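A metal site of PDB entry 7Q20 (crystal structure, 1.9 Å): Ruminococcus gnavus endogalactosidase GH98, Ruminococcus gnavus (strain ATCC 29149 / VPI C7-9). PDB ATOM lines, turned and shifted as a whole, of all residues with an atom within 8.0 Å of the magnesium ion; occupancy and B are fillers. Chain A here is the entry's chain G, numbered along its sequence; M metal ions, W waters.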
ATOM      1  N   LEU A 501      13.781 -23.491 -18.406  1.00  0.00           N
ATOM      2  CA  LEU A 501      14.731 -22.467 -18.837  1.00  0.00           C
ATOM      3  C   LEU A 501      16.194 -22.897 -18.698  1.00  0.00           C
ATOM      4  O   LEU A 501      17.052 -22.384 -19.398  1.00  0.00           O
ATOM      5  CB  LEU A 501      14.496 -21.131 -18.103  1.00  0.00           C
ATOM      6  CG  LEU A 501      13.177 -20.455 -18.477  1.00  0.00           C
ATOM      7  CD1 LEU A 501      12.905 -19.331 -17.488  1.00  0.00           C
ATOM      8  CD2 LEU A 501      13.225 -19.921 -19.882  1.00  0.00           C
ATOM      9  N   GLU A 551      25.202 -19.810 -23.953  1.00  0.00           N
ATOM     10  CA  GLU A 551      24.851 -18.762 -22.978  1.00  0.00           C
ATOM     11  C   GLU A 551      25.673 -18.810 -21.682  1.00  0.00           C
ATOM     12  O   GLU A 551      25.740 -17.821 -20.963  1.00  0.00           O
ATOM     13  CB  GLU A 551      23.356 -18.843 -22.633  1.00  0.00           C
ATOM     14  CG  GLU A 551      22.454 -18.584 -23.839  1.00  0.00           C
ATOM     15  CD  GLU A 551      21.433 -17.495 -23.578  1.00  0.00           C
ATOM     16  OE1 GLU A 551      21.884 -16.364 -23.318  1.00  0.00           O
ATOM     17  OE2 GLU A 551      20.208 -17.774 -23.646  1.00  0.00           O
ATOM     18  N   GLY A 581      16.551 -14.478 -13.622  1.00  0.00           N
ATOM     19  CA  GLY A 581      17.048 -15.433 -14.613  1.00  0.00           C
ATOM     20  C   GLY A 581      18.324 -14.954 -15.301  1.00  0.00           C
ATOM     21  O   GLY A 581      18.775 -15.559 -16.253  1.00  0.00           O
ATOM     22  N   ARG A 582      18.918 -13.889 -14.785  1.00  0.00           N
ATOM     23  CA  ARG A 582      20.051 -13.172 -15.420  1.00  0.00           C
ATOM     24  C   ARG A 582      21.237 -14.128 -15.633  1.00  0.00           C
ATOM     25  O   ARG A 582      21.934 -13.998 -16.666  1.00  0.00           O
ATOM     26  CB  ARG A 582      20.481 -12.009 -14.523  1.00  0.00           C
ATOM     27  CG  ARG A 582      21.644 -11.202 -15.090  1.00  0.00           C
ATOM     28  CD  ARG A 582      21.929 -10.015 -14.196  1.00  0.00           C
ATOM     29  NE  ARG A 582      23.070  -9.261 -14.660  1.00  0.00           N
ATOM     30  CZ  ARG A 582      23.452  -8.084 -14.156  1.00  0.00           C
ATOM     31  NH1 ARG A 582      22.782  -7.533 -13.160  1.00  0.00           N
ATOM     32  NH2 ARG A 582      24.505  -7.466 -14.658  1.00  0.00           N
ATOM     33  N   TYR A 583      21.475 -15.009 -14.666  1.00  0.00           N
ATOM     34  CA  TYR A 583      22.673 -15.886 -14.628  1.00  0.00           C
ATOM     35  C   TYR A 583      22.295 -17.322 -15.021  1.00  0.00           C
ATOM     36  O   TYR A 583      23.199 -18.158 -15.082  1.00  0.00           O
ATOM     37  CB  TYR A 583      23.320 -15.808 -13.242  1.00  0.00           C
ATOM     38  CG  TYR A 583      23.474 -14.404 -12.703  1.00  0.00           C
ATOM     39  CD1 TYR A 583      24.405 -13.531 -13.242  1.00  0.00           C
ATOM     40  CD2 TYR A 583      22.673 -13.939 -11.675  1.00  0.00           C
ATOM     41  CE1 TYR A 583      24.539 -12.235 -12.773  1.00  0.00           C
ATOM     42  CE2 TYR A 583      22.805 -12.646 -11.184  1.00  0.00           C
ATOM     43  CZ  TYR A 583      23.742 -11.792 -11.734  1.00  0.00           C
ATOM     44  OH  TYR A 583      23.886 -10.526 -11.255  1.00  0.00           O
ATOM     45  N   GLY A 584      21.010 -17.597 -15.271  1.00  0.00           N
ATOM     46  CA  GLY A 584      20.521 -18.950 -15.451  1.00  0.00           C
ATOM     47  C   GLY A 584      20.663 -19.759 -14.172  1.00  0.00           C
ATOM     48  O   GLY A 584      20.673 -19.198 -13.052  1.00  0.00           O
ATOM     49  N   TYR A 637      27.425 -11.477 -17.491  1.00  0.00           N
ATOM     50  CA  TYR A 637      25.982 -11.605 -17.823  1.00  0.00           C
ATOM     51  C   TYR A 637      25.315 -10.241 -17.720  1.00  0.00           C
ATOM     52  O   TYR A 637      25.117  -9.725 -16.623  1.00  0.00           O
ATOM     53  CB  TYR A 637      25.322 -12.633 -16.899  1.00  0.00           C
ATOM     54  CG  TYR A 637      25.885 -14.030 -17.012  1.00  0.00           C
ATOM     55  CD1 TYR A 637      25.516 -14.875 -18.043  1.00  0.00           C
ATOM     56  CD2 TYR A 637      26.789 -14.508 -16.082  1.00  0.00           C
ATOM     57  CE1 TYR A 637      26.054 -16.148 -18.159  1.00  0.00           C
ATOM     58  CE2 TYR A 637      27.325 -15.784 -16.175  1.00  0.00           C
ATOM     59  CZ  TYR A 637      26.952 -16.607 -17.217  1.00  0.00           C
ATOM     60  OH  TYR A 637      27.478 -17.867 -17.310  1.00  0.00           O
ATOM     61  N   PRO A 638      24.987  -9.568 -18.855  1.00  0.00           N
ATOM     62  CA  PRO A 638      24.361  -8.245 -18.813  1.00  0.00           C
ATOM     63  C   PRO A 638      22.936  -8.295 -18.230  1.00  0.00           C
ATOM     64  O   PRO A 638      22.255  -9.298 -18.384  1.00  0.00           O
ATOM     65  CB  PRO A 638      24.316  -7.792 -20.280  1.00  0.00           C
ATOM     66  CG  PRO A 638      25.278  -8.718 -20.995  1.00  0.00           C
ATOM     67  CD  PRO A 638      25.210 -10.027 -20.224  1.00  0.00           C
ATOM     68  N   GLU A 640      19.057  -7.745 -18.005  1.00  0.00           N
ATOM     69  CA  GLU A 640      17.988  -7.798 -19.018  1.00  0.00           C
ATOM     70  C   GLU A 640      16.733  -6.972 -18.651  1.00  0.00           C
ATOM     71  O   GLU A 640      15.990  -6.568 -19.548  1.00  0.00           O
ATOM     72  CB  GLU A 640      17.540  -9.235 -19.297  1.00  0.00           C
ATOM     73  CG  GLU A 640      18.677 -10.184 -19.653  1.00  0.00           C
ATOM     74  CD  GLU A 640      18.205 -11.582 -20.012  1.00  0.00           C
ATOM     75  OE1 GLU A 640      17.339 -12.146 -19.315  1.00  0.00           O
ATOM     76  OE2 GLU A 640      18.684 -12.135 -21.007  1.00  0.00           O
ATOM     77  N   ALA A 647      12.387 -12.615 -13.916  1.00  0.00           N
ATOM     78  CA  ALA A 647      12.172 -12.520 -15.361  1.00  0.00           C
ATOM     79  C   ALA A 647      13.413 -13.066 -16.057  1.00  0.00           C
ATOM     80  O   ALA A 647      14.518 -12.968 -15.526  1.00  0.00           O
ATOM     81  CB  ALA A 647      11.928 -11.078 -15.786  1.00  0.00           C
ATOM     82  N   ASP A 648      13.203 -13.651 -17.245  1.00  0.00           N
ATOM     83  CA  ASP A 648      14.262 -14.123 -18.114  1.00  0.00           C
ATOM     84  C   ASP A 648      13.741 -13.958 -19.532  1.00  0.00           C
ATOM     85  O   ASP A 648      12.643 -14.423 -19.840  1.00  0.00           O
ATOM     86  CB  ASP A 648      14.562 -15.602 -17.847  1.00  0.00           C
ATOM     87  CG  ASP A 648      15.789 -16.127 -18.624  1.00  0.00           C
ATOM     88  OD1 ASP A 648      16.519 -15.352 -19.329  1.00  0.00           O
ATOM     89  OD2 ASP A 648      16.031 -17.353 -18.495  1.00  0.00           O
ATOM     90  N   LYS A 649      14.494 -13.251 -20.364  1.00  0.00           N
ATOM     91  CA  LYS A 649      14.264 -13.268 -21.797  1.00  0.00           C
ATOM     92  C   LYS A 649      15.145 -14.360 -22.426  1.00  0.00           C
ATOM     93  O   LYS A 649      16.381 -14.395 -22.212  1.00  0.00           O
ATOM     94  CB  LYS A 649      14.497 -11.890 -22.452  1.00  0.00           C
ATOM     95  CG  LYS A 649      13.903 -11.799 -23.856  1.00  0.00           C
ATOM     96  CD  LYS A 649      14.064 -10.448 -24.521  1.00  0.00           C
ATOM     97  CE  LYS A 649      13.218 -10.404 -25.788  1.00  0.00           C
ATOM     98  NZ  LYS A 649      13.279  -9.115 -26.504  1.00  0.00           N
ATOM     99  N   TRP A 650      14.492 -15.282 -23.134  1.00  0.00           N
ATOM    100  CA  TRP A 650      15.137 -16.395 -23.831  1.00  0.00           C
ATOM    101  C   TRP A 650      14.509 -16.589 -25.214  1.00  0.00           C
ATOM    102  O   TRP A 650      13.297 -16.847 -25.319  1.00  0.00           O
ATOM    103  CB  TRP A 650      15.105 -17.712 -22.996  1.00  0.00           C
ATOM    104  CG  TRP A 650      15.706 -18.807 -23.798  1.00  0.00           C
ATOM    105  CD1 TRP A 650      17.006 -18.884 -24.212  1.00  0.00           C
ATOM    106  CD2 TRP A 650      15.024 -19.926 -24.390  1.00  0.00           C
ATOM    107  NE1 TRP A 650      17.160 -19.986 -25.003  1.00  0.00           N
ATOM    108  CE2 TRP A 650      15.968 -20.630 -25.137  1.00  0.00           C
ATOM    109  CE3 TRP A 650      13.704 -20.379 -24.357  1.00  0.00           C
ATOM    110  CZ2 TRP A 650      15.638 -21.786 -25.855  1.00  0.00           C
ATOM    111  CZ3 TRP A 650      13.380 -21.520 -25.066  1.00  0.00           C
ATOM    112  CH2 TRP A 650      14.333 -22.210 -25.797  1.00  0.00           C
ATOM    113  N   GLU A 651      15.333 -16.456 -26.262  1.00  0.00           N
ATOM    114  CA  GLU A 651      14.924 -16.585 -27.668  1.00  0.00           C
ATOM    115  C   GLU A 651      13.572 -15.898 -27.971  1.00  0.00           C
ATOM    116  O   GLU A 651      12.602 -16.547 -28.395  1.00  0.00           O
ATOM    117  CB  GLU A 651      14.909 -18.057 -28.116  1.00  0.00           C
ATOM    118  CG  GLU A 651      16.305 -18.686 -28.245  1.00  0.00           C
ATOM    119  CD  GLU A 651      17.205 -18.031 -29.310  1.00  0.00           C
ATOM    120  OE1 GLU A 651      16.685 -17.342 -30.228  1.00  0.00           O
ATOM    121  OE2 GLU A 651      18.444 -18.190 -29.234  1.00  0.00           O
ATOM    122  N   THR A 653      11.300 -14.525 -26.056  1.00  0.00           N
ATOM    123  CA  THR A 653      10.163 -14.693 -25.159  1.00  0.00           C
ATOM    124  C   THR A 653      10.545 -14.340 -23.731  1.00  0.00           C
ATOM    125  O   THR A 653      11.594 -14.761 -23.260  1.00  0.00           O
ATOM    126  CB  THR A 653       9.625 -16.125 -25.258  1.00  0.00           C
ATOM    127  OG1 THR A 653       9.370 -16.435 -26.620  1.00  0.00           O
ATOM    128  CG2 THR A 653       8.334 -16.311 -24.463  1.00  0.00           C
ATOM    129  N   TRP A 654       9.701 -13.553 -23.048  1.00  0.00           N
ATOM    130  CA  TRP A 654       9.871 -13.258 -21.640  1.00  0.00           C
ATOM    131  C   TRP A 654       9.091 -14.256 -20.779  1.00  0.00           C
ATOM    132  O   TRP A 654       7.918 -14.538 -21.028  1.00  0.00           O
ATOM    133  CB  TRP A 654       9.386 -11.870 -21.298  1.00  0.00           C
ATOM    134  CG  TRP A 654      10.268 -10.779 -21.747  1.00  0.00           C
ATOM    135  CD1 TRP A 654      10.101 -10.020 -22.860  1.00  0.00           C
ATOM    136  CD2 TRP A 654      11.427 -10.284 -21.083  1.00  0.00           C
ATOM    137  NE1 TRP A 654      11.102  -9.075 -22.935  1.00  0.00           N
ATOM    138  CE2 TRP A 654      11.920  -9.212 -21.850  1.00  0.00           C
ATOM    139  CE3 TRP A 654      12.104 -10.643 -19.901  1.00  0.00           C
ATOM    140  CZ2 TRP A 654      13.071  -8.493 -21.482  1.00  0.00           C
ATOM    141  CZ3 TRP A 654      13.223  -9.931 -19.534  1.00  0.00           C
ATOM    142  CH2 TRP A 654      13.713  -8.869 -20.330  1.00  0.00           C
ATOM    143  N   TYR A 655       9.775 -14.781 -19.763  1.00  0.00           N
ATOM    144  CA  TYR A 655       9.252 -15.719 -18.738  1.00  0.00           C
ATOM    145  C   TYR A 655       9.379 -15.022 -17.380  1.00  0.00           C
ATOM    146  O   TYR A 655      10.500 -14.612 -17.064  1.00  0.00           O
ATOM    147  CB  TYR A 655      10.033 -17.027 -18.752  1.00  0.00           C
ATOM    148  CG  TYR A 655      10.020 -17.709 -20.101  1.00  0.00           C
ATOM    149  CD1 TYR A 655      10.914 -17.336 -21.092  1.00  0.00           C
ATOM    150  CD2 TYR A 655       9.110 -18.701 -20.390  1.00  0.00           C
ATOM    151  CE1 TYR A 655      10.904 -17.944 -22.334  1.00  0.00           C
ATOM    152  CE2 TYR A 655       9.073 -19.324 -21.633  1.00  0.00           C
ATOM    153  CZ  TYR A 655       9.973 -18.937 -22.617  1.00  0.00           C
ATOM    154  OH  TYR A 655       9.953 -19.505 -23.858  1.00  0.00           O
HETATM  155 MG    MG M   1      18.073 -14.476 -20.799  1.00  0.00          MG
HETATM  156  O   HOH W   1      18.292 -16.606 -21.584  1.00  0.00           O
HETATM  157  O   HOH W   2      19.119 -14.571 -19.073  1.00  0.00           O
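The backbone NH (N) of Asp 648 is in hydrogen-bond range of the backbone carbonyl oxygen (O) of Tyr 655 (2.9 Å).
Within 4 Å of the magnesium ion: Glu 640, Asp 648 and Lys 649.
The nearest printed residue that does not touch the magnesium ion is Trp 650 (4.4 Å).
The magnesium ion is bound by water W2 (2.0 Å), the backbone carbonyl oxygen of Lys 649 (2.2 Å), water W1 (2.3 Å), the side-chain carboxylate of Asp 648 (2.3 Å) and the side-chain carboxylate of Glu 640 (2.4 Å).
The magnesium ion has five donor atoms within binding distance.
Water W2 bridges the backbone carbonyl oxygen (O) of Gly 581 (3.0 Å) and the side-chain carboxylate (OE1) of Glu 640 (3.0 Å).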
